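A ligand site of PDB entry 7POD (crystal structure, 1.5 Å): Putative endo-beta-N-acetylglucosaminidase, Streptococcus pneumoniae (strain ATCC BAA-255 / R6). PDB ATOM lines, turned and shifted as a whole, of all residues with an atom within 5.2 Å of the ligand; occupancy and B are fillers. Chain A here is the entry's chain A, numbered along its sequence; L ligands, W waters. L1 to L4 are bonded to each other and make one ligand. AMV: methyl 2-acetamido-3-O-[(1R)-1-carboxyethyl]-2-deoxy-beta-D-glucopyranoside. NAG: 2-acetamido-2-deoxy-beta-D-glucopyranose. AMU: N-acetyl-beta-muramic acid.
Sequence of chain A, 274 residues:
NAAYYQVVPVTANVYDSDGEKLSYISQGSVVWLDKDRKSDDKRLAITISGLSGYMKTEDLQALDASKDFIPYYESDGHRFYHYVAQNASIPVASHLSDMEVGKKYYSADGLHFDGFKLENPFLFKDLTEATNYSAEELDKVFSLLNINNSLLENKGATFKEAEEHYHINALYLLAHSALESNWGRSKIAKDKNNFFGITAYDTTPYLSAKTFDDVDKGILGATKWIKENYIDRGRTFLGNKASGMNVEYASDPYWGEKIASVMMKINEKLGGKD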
ATOM      1  N   THR A  11      -3.005   7.198   8.368  1.00  0.00           N
ATOM      2  CA  THR A  11      -3.644   8.508   8.517  1.00  0.00           C
ATOM      3  C   THR A  11      -4.691   8.686   7.404  1.00  0.00           C
ATOM      4  O   THR A  11      -4.571   8.061   6.338  1.00  0.00           O
ATOM      5  CB  THR A  11      -2.620   9.670   8.479  1.00  0.00           C
ATOM      6  OG1 THR A  11      -2.022   9.790   7.184  1.00  0.00           O
ATOM      7  CG2 THR A  11      -1.549   9.531   9.533  1.00  0.00           C
ATOM      8  N   ASN A  13      -6.955  12.148   5.503  1.00  0.00           N
ATOM      9  CA  ASN A  13      -7.118  13.615   5.434  1.00  0.00           C
ATOM     10  C   ASN A  13      -8.565  14.016   5.744  1.00  0.00           C
ATOM     11  O   ASN A  13      -9.523  13.249   5.535  1.00  0.00           O
ATOM     12  CB  ASN A  13      -6.740  14.113   4.056  1.00  0.00           C
ATOM     13  CG  ASN A  13      -5.283  13.861   3.763  1.00  0.00           C
ATOM     14  OD1 ASN A  13      -4.440  13.859   4.668  1.00  0.00           O
ATOM     15  ND2 ASN A  13      -4.981  13.580   2.519  1.00  0.00           N
ATOM     16  N   TYR A  24      -5.157  16.202   8.890  1.00  0.00           N
ATOM     17  CA  TYR A  24      -5.045  14.719   8.783  1.00  0.00           C
ATOM     18  C   TYR A  24      -5.217  14.169  10.188  1.00  0.00           C
ATOM     19  O   TYR A  24      -4.858  14.876  11.180  1.00  0.00           O
ATOM     20  CB  TYR A  24      -3.709  14.308   8.159  1.00  0.00           C
ATOM     21  CG  TYR A  24      -2.491  14.679   8.980  1.00  0.00           C
ATOM     22  CD1 TYR A  24      -2.128  15.990   9.182  1.00  0.00           C
ATOM     23  CD2 TYR A  24      -1.703  13.710   9.564  1.00  0.00           C
ATOM     24  CE1 TYR A  24      -1.031  16.334   9.960  1.00  0.00           C
ATOM     25  CE2 TYR A  24      -0.577  14.034  10.314  1.00  0.00           C
ATOM     26  CZ  TYR A  24      -0.246  15.358  10.532  1.00  0.00           C
ATOM     27  OH  TYR A  24       0.851  15.650  11.337  1.00  0.00           O
ATOM     28  N   SER A  26      -5.248  10.340  12.722  1.00  0.00           N
ATOM     29  CA  SER A  26      -4.605   9.023  12.909  1.00  0.00           C
ATOM     30  C   SER A  26      -5.600   7.874  12.756  1.00  0.00           C
ATOM     31  O   SER A  26      -6.796   7.964  13.116  1.00  0.00           O
ATOM     32  CB  SER A  26      -3.938   8.958  14.248  1.00  0.00           C
ATOM     33  OG  SER A  26      -4.864   9.253  15.259  1.00  0.00           O
ATOM     34  N   LEU A 179       5.253  14.270  27.020  1.00  0.00           N
ATOM     35  CA  LEU A 179       4.206  13.508  26.291  1.00  0.00           C
ATOM     36  C   LEU A 179       4.847  12.756  25.124  1.00  0.00           C
ATOM     37  O   LEU A 179       4.618  11.550  24.954  1.00  0.00           O
ATOM     38  CB  LEU A 179       3.110  14.459  25.778  1.00  0.00           C
ATOM     39  CG  LEU A 179       2.104  13.632  24.985  1.00  0.00           C
ATOM     40  CD1 LEU A 179       1.223  12.829  25.958  1.00  0.00           C
ATOM     41  CD2 LEU A 179       1.389  14.320  23.878  1.00  0.00           C
ATOM     42  N   GLU A 180       5.601  13.465  24.283  1.00  0.00           N
ATOM     43  CA  GLU A 180       5.993  12.925  22.972  1.00  0.00           C
ATOM     44  C   GLU A 180       7.011  11.780  23.124  1.00  0.00           C
ATOM     45  O   GLU A 180       7.006  10.863  22.311  1.00  0.00           O
ATOM     46  CB  GLU A 180       6.528  14.033  22.069  1.00  0.00           C
ATOM     47  CG  GLU A 180       6.372  13.644  20.625  1.00  0.00           C
ATOM     48  CD  GLU A 180       5.258  14.273  19.807  1.00  0.00           C
ATOM     49  OE1 GLU A 180       5.029  15.460  19.964  1.00  0.00           O
ATOM     50  OE2 GLU A 180       4.830  13.650  18.849  1.00  0.00           O
ATOM     51  N   SER A 181       7.871  11.837  24.150  1.00  0.00           N
ATOM     52  CA  SER A 181       9.040  10.931  24.275  1.00  0.00           C
ATOM     53  C   SER A 181       8.957  10.123  25.555  1.00  0.00           C
ATOM     54  O   SER A 181       9.935   9.547  25.950  1.00  0.00           O
ATOM     55  CB  SER A 181      10.347  11.671  24.152  1.00  0.00           C
ATOM     56  OG  SER A 181      10.589  12.475  25.279  1.00  0.00           O
ATOM     57  N   ASN A 182       7.800  10.114  26.219  1.00  0.00           N
ATOM     58  CA  ASN A 182       7.645   9.420  27.519  1.00  0.00           C
ATOM     59  C   ASN A 182       8.711   9.930  28.507  1.00  0.00           C
ATOM     60  O   ASN A 182       9.523   9.137  28.976  1.00  0.00           O
ATOM     61  CB  ASN A 182       7.657   7.905  27.359  1.00  0.00           C
ATOM     62  CG  ASN A 182       7.463   7.210  28.682  1.00  0.00           C
ATOM     63  OD1 ASN A 182       6.875   7.770  29.607  1.00  0.00           O
ATOM     64  ND2 ASN A 182       8.030   6.022  28.816  1.00  0.00           N
ATOM     65  N   SER A 186      11.721   7.193  25.501  1.00  0.00           N
ATOM     66  CA  SER A 186      11.384   6.450  24.271  1.00  0.00           C
ATOM     67  C   SER A 186      12.681   6.048  23.544  1.00  0.00           C
ATOM     68  O   SER A 186      13.779   6.566  23.816  1.00  0.00           O
ATOM     69  CB  SER A 186      10.526   7.216  23.354  1.00  0.00           C
ATOM     70  OG  SER A 186      11.242   8.299  22.818  1.00  0.00           O
ATOM     71  N   ILE A 188      13.385   6.674  20.411  1.00  0.00           N
ATOM     72  CA  ILE A 188      13.762   7.907  19.651  1.00  0.00           C
ATOM     73  C   ILE A 188      14.507   8.848  20.622  1.00  0.00           C
ATOM     74  O   ILE A 188      15.563   9.394  20.238  1.00  0.00           O
ATOM     75  CB  ILE A 188      12.491   8.519  18.987  1.00  0.00           C
ATOM     76  CG1 ILE A 188      11.991   7.603  17.841  1.00  0.00           C
ATOM     77  CG2 ILE A 188      12.699   9.901  18.443  1.00  0.00           C
ATOM     78  CD1 ILE A 188      10.666   8.009  17.175  1.00  0.00           C
ATOM     79  N   PHE A 196      10.910  15.373  21.110  1.00  0.00           N
ATOM     80  CA  PHE A 196       9.750  16.155  20.609  1.00  0.00           C
ATOM     81  C   PHE A 196       9.152  15.517  19.352  1.00  0.00           C
ATOM     82  O   PHE A 196       8.293  16.163  18.742  1.00  0.00           O
ATOM     83  CB  PHE A 196      10.148  17.606  20.348  1.00  0.00           C
ATOM     84  CG  PHE A 196      10.598  18.364  21.572  1.00  0.00           C
ATOM     85  CD1 PHE A 196      11.890  18.204  22.074  1.00  0.00           C
ATOM     86  CD2 PHE A 196       9.713  19.197  22.240  1.00  0.00           C
ATOM     87  CE1 PHE A 196      12.314  18.927  23.159  1.00  0.00           C
ATOM     88  CE2 PHE A 196      10.132  19.906  23.358  1.00  0.00           C
ATOM     89  CZ  PHE A 196      11.422  19.754  23.824  1.00  0.00           C
ATOM     90  N   GLY A 197       9.573  14.308  18.982  1.00  0.00           N
ATOM     91  CA  GLY A 197       9.053  13.656  17.757  1.00  0.00           C
ATOM     92  C   GLY A 197       9.354  14.453  16.497  1.00  0.00           C
ATOM     93  O   GLY A 197       8.544  14.371  15.547  1.00  0.00           O
ATOM     94  N   ILE A 198      10.474  15.189  16.454  1.00  0.00           N
ATOM     95  CA  ILE A 198      10.814  15.999  15.260  1.00  0.00           C
ATOM     96  C   ILE A 198      10.993  15.042  14.081  1.00  0.00           C
ATOM     97  O   ILE A 198      11.896  14.192  14.158  1.00  0.00           O
ATOM     98  CB  ILE A 198      12.044  16.905  15.471  1.00  0.00           C
ATOM     99  CG1 ILE A 198      11.993  17.809  16.725  1.00  0.00           C
ATOM    100  CG2 ILE A 198      12.301  17.710  14.231  1.00  0.00           C
ATOM    101  CD1 ILE A 198      10.980  18.844  16.687  1.00  0.00           C
ATOM    102  N   THR A 199      10.180  15.308  13.023  1.00  0.00           N
ATOM    103  CA  THR A 199      10.025  14.556  11.746  1.00  0.00           C
ATOM    104  C   THR A 199       9.797  13.061  12.012  1.00  0.00           C
ATOM    105  O   THR A 199      10.140  12.263  11.165  1.00  0.00           O
ATOM    106  CB  THR A 199      11.176  14.837  10.792  1.00  0.00           C
ATOM    107  OG1 THR A 199      12.425  14.242  11.168  1.00  0.00           O
ATOM    108  CG2 THR A 199      11.367  16.323  10.586  1.00  0.00           C
ATOM    109  N   ALA A 200       9.156  12.701  13.118  1.00  0.00           N
ATOM    110  CA  ALA A 200       8.826  11.287  13.459  1.00  0.00           C
ATOM    111  C   ALA A 200       7.494  10.911  12.793  1.00  0.00           C
ATOM    112  O   ALA A 200       6.457  10.707  13.529  1.00  0.00           O
ATOM    113  CB  ALA A 200       8.760  11.083  14.953  1.00  0.00           C
ATOM    114  N   TYR A 201       7.494  10.872  11.466  1.00  0.00           N
ATOM    115  CA  TYR A 201       6.267  10.747  10.655  1.00  0.00           C
ATOM    116  C   TYR A 201       5.564   9.414  10.955  1.00  0.00           C
ATOM    117  O   TYR A 201       6.262   8.397  11.102  1.00  0.00           O
ATOM    118  CB  TYR A 201       6.619  10.807   9.149  1.00  0.00           C
ATOM    119  CG  TYR A 201       7.336  12.060   8.726  1.00  0.00           C
ATOM    120  CD1 TYR A 201       6.981  13.283   9.246  1.00  0.00           C
ATOM    121  CD2 TYR A 201       8.379  12.008   7.808  1.00  0.00           C
ATOM    122  CE1 TYR A 201       7.634  14.454   8.863  1.00  0.00           C
ATOM    123  CE2 TYR A 201       9.028  13.165   7.400  1.00  0.00           C
ATOM    124  CZ  TYR A 201       8.663  14.390   7.938  1.00  0.00           C
ATOM    125  OH  TYR A 201       9.297  15.527   7.592  1.00  0.00           O
ATOM    126  N   ASP A 202       4.233   9.393  10.881  1.00  0.00           N
ATOM    127  CA  ASP A 202       3.409   8.210  11.239  1.00  0.00           C
ATOM    128  C   ASP A 202       3.845   6.971  10.443  1.00  0.00           C
ATOM    129  O   ASP A 202       3.793   5.834  10.998  1.00  0.00           O
ATOM    130  CB  ASP A 202       1.928   8.443  10.947  1.00  0.00           C
ATOM    131  CG  ASP A 202       1.269   9.520  11.791  1.00  0.00           C
ATOM    132  OD1 ASP A 202       1.619  10.697  11.594  1.00  0.00           O
ATOM    133  OD2 ASP A 202       0.363   9.170  12.553  1.00  0.00           O
ATOM    134  N   THR A 203       4.210   7.161   9.174  1.00  0.00           N
ATOM    135  CA  THR A 203       4.539   6.029   8.254  1.00  0.00           C
ATOM    136  C   THR A 203       5.764   5.291   8.799  1.00  0.00           C
ATOM    137  O   THR A 203       5.755   4.043   8.778  1.00  0.00           O
ATOM    138  CB  THR A 203       4.645   6.534   6.805  1.00  0.00           C
ATOM    139  OG1 THR A 203       4.722   5.417   5.927  1.00  0.00           O
ATOM    140  CG2 THR A 203       5.824   7.450   6.574  1.00  0.00           C
ATOM    141  N   PRO A 205       8.067   6.278  12.011  1.00  0.00           N
ATOM    142  CA  PRO A 205       8.388   7.301  13.014  1.00  0.00           C
ATOM    143  C   PRO A 205       9.855   7.262  13.467  1.00  0.00           C
ATOM    144  O   PRO A 205      10.489   8.320  13.472  1.00  0.00           O
ATOM    145  CB  PRO A 205       7.438   7.022  14.194  1.00  0.00           C
ATOM    146  CG  PRO A 205       6.436   6.010  13.694  1.00  0.00           C
ATOM    147  CD  PRO A 205       7.009   5.358  12.447  1.00  0.00           C
ATOM    148  N   TRP A 225      13.569  24.293  16.102  1.00  0.00           N
ATOM    149  CA  TRP A 225      12.797  23.683  14.986  1.00  0.00           C
ATOM    150  C   TRP A 225      11.321  24.064  15.167  1.00  0.00           C
ATOM    151  O   TRP A 225      10.658  24.494  14.202  1.00  0.00           O
ATOM    152  CB  TRP A 225      12.996  22.169  14.976  1.00  0.00           C
ATOM    153  CG  TRP A 225      12.434  21.502  13.776  1.00  0.00           C
ATOM    154  CD1 TRP A 225      13.154  21.123  12.680  1.00  0.00           C
ATOM    155  CD2 TRP A 225      11.084  21.114  13.526  1.00  0.00           C
ATOM    156  NE1 TRP A 225      12.337  20.575  11.719  1.00  0.00           N
ATOM    157  CE2 TRP A 225      11.069  20.524  12.233  1.00  0.00           C
ATOM    158  CE3 TRP A 225       9.901  21.159  14.240  1.00  0.00           C
ATOM    159  CZ2 TRP A 225       9.908  20.037  11.648  1.00  0.00           C
ATOM    160  CZ3 TRP A 225       8.750  20.655  13.662  1.00  0.00           C
ATOM    161  CH2 TRP A 225       8.756  20.068  12.404  1.00  0.00           C
ATOM    162  N   TYR A 230       6.739  26.332  13.390  1.00  0.00           N
ATOM    163  CA  TYR A 230       5.379  26.497  13.962  1.00  0.00           C
ATOM    164  C   TYR A 230       5.165  27.933  14.464  1.00  0.00           C
ATOM    165  O   TYR A 230       4.279  28.632  13.904  1.00  0.00           O
ATOM    166  CB  TYR A 230       5.135  25.414  15.014  1.00  0.00           C
ATOM    167  CG  TYR A 230       4.814  24.104  14.365  1.00  0.00           C
ATOM    168  CD1 TYR A 230       5.840  23.263  13.924  1.00  0.00           C
ATOM    169  CD2 TYR A 230       3.513  23.781  14.022  1.00  0.00           C
ATOM    170  CE1 TYR A 230       5.555  22.107  13.203  1.00  0.00           C
ATOM    171  CE2 TYR A 230       3.224  22.618  13.322  1.00  0.00           C
ATOM    172  CZ  TYR A 230       4.235  21.772  12.919  1.00  0.00           C
ATOM    173  OH  TYR A 230       3.914  20.650  12.187  1.00  0.00           O
ATOM    174  N   GLU A 248      -1.170  20.625  12.136  1.00  0.00           N
ATOM    175  CA  GLU A 248      -0.058  20.049  11.344  1.00  0.00           C
ATOM    176  C   GLU A 248       0.871  19.136  12.162  1.00  0.00           C
ATOM    177  O   GLU A 248       1.499  18.240  11.504  1.00  0.00           O
ATOM    178  CB  GLU A 248       0.739  21.142  10.656  1.00  0.00           C
ATOM    179  CG  GLU A 248      -0.124  22.023   9.785  1.00  0.00           C
ATOM    180  CD  GLU A 248      -0.603  23.302  10.438  1.00  0.00           C
ATOM    181  OE1 GLU A 248      -0.312  23.528  11.650  1.00  0.00           O
ATOM    182  OE2 GLU A 248      -1.275  24.082   9.705  1.00  0.00           O
ATOM    183  N   TYR A 249       1.028  19.341  13.484  1.00  0.00           N
ATOM    184  CA  TYR A 249       2.193  18.769  14.189  1.00  0.00           C
ATOM    185  C   TYR A 249       2.036  17.243  14.279  1.00  0.00           C
ATOM    186  O   TYR A 249       3.028  16.516  14.224  1.00  0.00           O
ATOM    187  CB  TYR A 249       2.374  19.399  15.582  1.00  0.00           C
ATOM    188  CG  TYR A 249       3.736  19.118  16.167  1.00  0.00           C
ATOM    189  CD1 TYR A 249       4.070  17.953  16.846  1.00  0.00           C
ATOM    190  CD2 TYR A 249       4.738  20.049  16.020  1.00  0.00           C
ATOM    191  CE1 TYR A 249       5.361  17.716  17.309  1.00  0.00           C
ATOM    192  CE2 TYR A 249       5.984  19.875  16.555  1.00  0.00           C
ATOM    193  CZ  TYR A 249       6.332  18.695  17.175  1.00  0.00           C
ATOM    194  OH  TYR A 249       7.639  18.571  17.591  1.00  0.00           O
ATOM    195  N   ALA A 250       0.814  16.773  14.486  1.00  0.00           N
ATOM    196  CA  ALA A 250       0.558  15.340  14.823  1.00  0.00           C
ATOM    197  C   ALA A 250      -0.775  14.905  14.254  1.00  0.00           C
ATOM    198  O   ALA A 250      -1.726  15.698  14.258  1.00  0.00           O
ATOM    199  CB  ALA A 250       0.530  15.114  16.328  1.00  0.00           C
ATOM    200  N   SER A 251      -0.851  13.641  13.841  1.00  0.00           N
ATOM    201  CA  SER A 251      -2.119  13.063  13.342  1.00  0.00           C
ATOM    202  C   SER A 251      -3.105  12.864  14.495  1.00  0.00           C
ATOM    203  O   SER A 251      -4.302  12.930  14.259  1.00  0.00           O
ATOM    204  CB  SER A 251      -1.880  11.770  12.671  1.00  0.00           C
ATOM    205  OG  SER A 251      -1.306  10.832  13.581  1.00  0.00           O
ATOM    206  N   ASP A 252      -2.587  12.641  15.696  1.00  0.00           N
ATOM    207  CA  ASP A 252      -3.427  12.436  16.897  1.00  0.00           C
ATOM    208  C   ASP A 252      -4.308  13.665  17.112  1.00  0.00           C
ATOM    209  O   ASP A 252      -3.820  14.758  17.412  1.00  0.00           O
ATOM    210  CB  ASP A 252      -2.501  12.227  18.082  1.00  0.00           C
ATOM    211  CG  ASP A 252      -3.177  11.976  19.412  1.00  0.00           C
ATOM    212  OD1 ASP A 252      -4.418  12.080  19.482  1.00  0.00           O
ATOM    213  OD2 ASP A 252      -2.421  11.616  20.355  1.00  0.00           O
ATOM    214  N   TRP A 255      -3.550  15.353  20.543  1.00  0.00           N
ATOM    215  CA  TRP A 255      -2.145  15.708  20.873  1.00  0.00           C
ATOM    216  C   TRP A 255      -2.115  16.986  21.718  1.00  0.00           C
ATOM    217  O   TRP A 255      -1.409  17.013  22.774  1.00  0.00           O
ATOM    218  CB  TRP A 255      -1.329  15.833  19.573  1.00  0.00           C
ATOM    219  CG  TRP A 255       0.069  16.365  19.713  1.00  0.00           C
ATOM    220  CD1 TRP A 255       1.231  15.661  19.888  1.00  0.00           C
ATOM    221  CD2 TRP A 255       0.454  17.735  19.635  1.00  0.00           C
ATOM    222  NE1 TRP A 255       2.303  16.512  19.866  1.00  0.00           N
ATOM    223  CE2 TRP A 255       1.859  17.794  19.724  1.00  0.00           C
ATOM    224  CE3 TRP A 255      -0.248  18.927  19.437  1.00  0.00           C
ATOM    225  CZ2 TRP A 255       2.549  19.015  19.713  1.00  0.00           C
ATOM    226  CZ3 TRP A 255       0.430  20.121  19.410  1.00  0.00           C
ATOM    227  CH2 TRP A 255       1.810  20.168  19.566  1.00  0.00           C
ATOM    228  N   LYS A 258      -3.534  16.438  25.147  1.00  0.00           N
ATOM    229  CA  LYS A 258      -2.595  15.624  25.952  1.00  0.00           C
ATOM    230  C   LYS A 258      -1.451  16.474  26.510  1.00  0.00           C
ATOM    231  O   LYS A 258      -1.095  16.316  27.684  1.00  0.00           O
ATOM    232  CB  LYS A 258      -2.029  14.462  25.154  1.00  0.00           C
ATOM    233  CG  LYS A 258      -3.046  13.377  24.858  1.00  0.00           C
ATOM    234  CD  LYS A 258      -2.510  12.360  23.860  1.00  0.00           C
ATOM    235  CE  LYS A 258      -3.406  11.180  23.638  1.00  0.00           C
ATOM    236  NZ  LYS A 258      -2.821  10.234  22.650  1.00  0.00           N
HETATM  237  C1  AMV L   1       2.991   9.708  21.866  1.00  0.00           C
HETATM  238  C2  AMV L   1       3.972   9.130  20.840  1.00  0.00           C
HETATM  239  C3  AMV L   1       4.259  10.199  19.779  1.00  0.00           C
HETATM  240  C4  AMV L   1       2.905  10.702  19.181  1.00  0.00           C
HETATM  241  C5  AMV L   1       1.984  11.159  20.307  1.00  0.00           C
HETATM  242  C6  AMV L   1       0.671  11.668  19.754  1.00  0.00           C
HETATM  243  C7  AMV L   1       5.519   7.546  22.101  1.00  0.00           C
HETATM  244  C8  AMV L   1       6.811   7.458  22.988  1.00  0.00           C
HETATM  245  C9  AMV L   1       6.583   9.614  19.100  1.00  0.00           C
HETATM  246  C10 AMV L   1       7.197   8.137  19.272  1.00  0.00           C
HETATM  247  C11 AMV L   1       7.139  10.555  18.062  1.00  0.00           C
HETATM  248  O1  AMV L   1       2.706   8.734  22.851  1.00  0.00           O
HETATM  249  O3  AMV L   1       5.126   9.678  18.754  1.00  0.00           O
HETATM  250  O4  AMV L   1       3.005  11.802  18.198  1.00  0.00           O
HETATM  251  O5  AMV L   1       1.789  10.091  21.235  1.00  0.00           O
HETATM  252  O6  AMV L   1      -0.075  12.138  20.839  1.00  0.00           O
HETATM  253  O7  AMV L   1       4.798   6.596  21.764  1.00  0.00           O
HETATM  254  O11 AMV L   1       8.290   7.829  19.973  1.00  0.00           O
HETATM  255  N2  AMV L   1       5.135   8.866  21.634  1.00  0.00           N
HETATM  256  C12 AMV L   1       2.128   9.185  24.099  1.00  0.00           C
HETATM  257  OXT AMV L   1       6.474   7.132  18.834  1.00  0.00           O
HETATM  258  C1  NAG L   2       3.604  11.571  16.886  1.00  0.00           C
HETATM  259  C2  NAG L   2       2.528  11.639  15.788  1.00  0.00           C
HETATM  260  C3  NAG L   2       2.937  11.969  14.315  1.00  0.00           C
HETATM  261  C4  NAG L   2       3.928  13.181  14.266  1.00  0.00           C
HETATM  262  C5  NAG L   2       4.985  13.181  15.347  1.00  0.00           C
HETATM  263  C6  NAG L   2       5.239  14.665  15.738  1.00  0.00           C
HETATM  264  C7  NAG L   2       0.368  10.498  16.202  1.00  0.00           C
HETATM  265  C8  NAG L   2      -0.470   9.202  16.274  1.00  0.00           C
HETATM  266  N2  NAG L   2       1.760  10.388  15.838  1.00  0.00           N
HETATM  267  O3  NAG L   2       1.745  12.280  13.615  1.00  0.00           O
HETATM  268  O4  NAG L   2       4.591  13.332  12.982  1.00  0.00           O
HETATM  269  O5  NAG L   2       4.515  12.651  16.573  1.00  0.00           O
HETATM  270  O6  NAG L   2       4.015  14.943  16.297  1.00  0.00           O
HETATM  271  O7  NAG L   2      -0.021  11.591  16.392  1.00  0.00           O
HETATM  272  C1  AMU L   3       3.897  14.030  11.898  1.00  0.00           C
HETATM  273  C2  AMU L   3       4.815  15.149  11.369  1.00  0.00           C
HETATM  274  C3  AMU L   3       4.111  15.813  10.190  1.00  0.00           C
HETATM  275  C4  AMU L   3       3.844  14.755   9.081  1.00  0.00           C
HETATM  276  C5  AMU L   3       3.006  13.613   9.681  1.00  0.00           C
HETATM  277  C6  AMU L   3       2.964  12.395   8.790  1.00  0.00           C
HETATM  278  C7  AMU L   3       6.427  16.567  12.727  1.00  0.00           C
HETATM  279  C8  AMU L   3       6.502  17.567  13.849  1.00  0.00           C
HETATM  280  C9  AMU L   3       4.443  18.167   9.879  1.00  0.00           C
HETATM  281  C10 AMU L   3       5.717  18.956   9.745  1.00  0.00           C
HETATM  282  C11 AMU L   3       3.385  18.633   8.852  1.00  0.00           C
HETATM  283  O3  AMU L   3       4.898  16.848   9.674  1.00  0.00           O
HETATM  284  O4  AMU L   3       3.140  15.324   8.002  1.00  0.00           O
HETATM  285  O5  AMU L   3       3.601  13.168  10.861  1.00  0.00           O
HETATM  286  O6  AMU L   3       2.054  11.455   9.264  1.00  0.00           O
HETATM  287  O7  AMU L   3       7.432  16.192  12.158  1.00  0.00           O
HETATM  288  O10 AMU L   3       6.686  18.585   8.938  1.00  0.00           O
HETATM  289  O11 AMU L   3       5.729  20.004  10.415  1.00  0.00           O
HETATM  290  N2  AMU L   3       5.084  16.137  12.393  1.00  0.00           N
HETATM  291  C1  NAG L   4       3.761  15.052   6.740  1.00  0.00           C
HETATM  292  C2  NAG L   4       2.644  15.349   5.717  1.00  0.00           C
HETATM  293  C3  NAG L   4       3.246  15.384   4.328  1.00  0.00           C
HETATM  294  C4  NAG L   4       4.478  16.294   4.277  1.00  0.00           C
HETATM  295  C5  NAG L   4       5.542  15.934   5.344  1.00  0.00           C
HETATM  296  C6  NAG L   4       6.711  16.946   5.479  1.00  0.00           C
HETATM  297  C7  NAG L   4       0.204  14.488   6.079  1.00  0.00           C
HETATM  298  C8  NAG L   4      -0.690  13.215   6.198  1.00  0.00           C
HETATM  299  N2  NAG L   4       1.632  14.283   5.823  1.00  0.00           N
HETATM  300  O3  NAG L   4       2.226  15.756   3.376  1.00  0.00           O
HETATM  301  O4  NAG L   4       5.007  16.205   2.960  1.00  0.00           O
HETATM  302  O5  NAG L   4       4.879  15.913   6.583  1.00  0.00           O
HETATM  303  O6  NAG L   4       6.269  18.198   6.074  1.00  0.00           O
HETATM  304  O7  NAG L   4      -0.234  15.584   6.195  1.00  0.00           O
HETATM  305  O   HOH W   1       3.359   9.668   7.677  1.00  0.00           O
HETATM  306  O   HOH W   2      10.481   5.756  20.164  1.00  0.00           O
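O of Ala 200 lies close to O4 of NAG L2 (3.3 Å). OG1 of Thr 11 touches C8 of NAG L4, 3.8 Å away. OH of Tyr 24 touches C5 of AMU L3, 3.4 Å away. O of Leu 179 touches C12 of AMV L1, 3.5 Å away. CB of Ser 186 touches C8 of AMV L1, 3.7 Å away. CD1 of Ile 188 touches O11 of AMV L1, at 3.7 Å. O of Gly 197 touches C6 of NAG L2, at 3.3 Å. Tyr 201 touches the ligand. CH2 of Trp 225 touches O11 of AMU L3, 3.6 Å away. O of Glu 248 touches C11 of AMU L3, 3.3 Å away. Ala 250 touches the ligand. Trp 255 touches the ligand. Lys 258 touches the ligand. Hydrophobic or aromatic side chains within 4 Å of the ligand: Tyr 24, Ile 188, Ala 200, Tyr 201, Trp 225, Tyr 230, Tyr 249, Ala 250 and Trp 255. Of the 28 residues printed, 20 come within 4 Å of the ligand. The nearest printed residue that does not touch the ligand is Ser 26 (4.02 Å).
Water W1 lies within hydrogen-bond range of an oxygen (O6) of AMU L3, the backbone NH of Thr 203 and the backbone NH of Asp 202. Water W2 bridges O11 of AMV L1 (3.0 Å) and N of Ile 188 (3.1 Å).
The side-chain hydroxyl (OH) of Tyr 230 sits close to the backbone NH (N) of Tyr 249. OD2 of Asp 252 is in salt-bridge range of NZ of Lys 258 (2.7 Å). N of Ser 186 lies within hydrogen-bond range of O of Ser 181 (3.0 Å). The backbone carbonyl oxygen of Glu 248 lies within hydrogen-bond range of the side-chain hydroxyl of Tyr 24 (2.7 Å). The side-chain hydroxyl (OH) of Tyr 24 sits at hydrogen-bond distance from the backbone NH (N) of Ala 250, at 3.3 Å. The side-chain carboxylate (OD2) of Asp 202 is in hydrogen-bond range of the side-chain hydroxyl (OG) of Ser 251. O of Glu 248 sits close to OH of Tyr 230, at 3.5 Å. The indole nitrogen (NE1) of Trp 255 lies within hydrogen-bond range of the side-chain carboxylate (OE1) of Glu 180, 2.9 Å away.
An oxygen (O6) of AMU L3 is in hydrogen-bond range of the side-chain carboxylate (OD1) of Asp 202, at 2.5 Å. An oxygen (O3) of NAG L2 is in hydrogen-bond range of the backbone NH of Ser 251, 2.9 Å away. The backbone NH (N) of Thr 199 sits at hydrogen-bond distance from an oxygen (O7) of AMU L3, 3.0 Å away. An oxygen (O7) of NAG L2 is in hydrogen-bond range of the backbone NH (N) of Asp 252 (2.9 Å). O6 of AMU L3 lies close to N of Asp 202 (3.4 Å). A nitrogen (N2) of AMV L1 lies within hydrogen-bond range of the backbone carbonyl oxygen of Glu 180, 2.8 Å away. OE2 of Glu 180 sits at hydrogen-bond distance from O6 of NAG L2, 3.0 Å away. The side-chain hydroxyl (OH) of Tyr 230 is in hydrogen-bond range of an oxygen (O11) of AMU L3, at 2.6 Å. The side-chain carboxylate (OD2) of Asp 252 lies within hydrogen-bond range of an oxygen (O6) of AMV L1, 2.5 Å away. O of Tyr 249 lies within hydrogen-bond range of N2 of AMU L3 (2.8 Å). OG of Ser 251 sits close to O7 of NAG L2 (3.2 Å).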
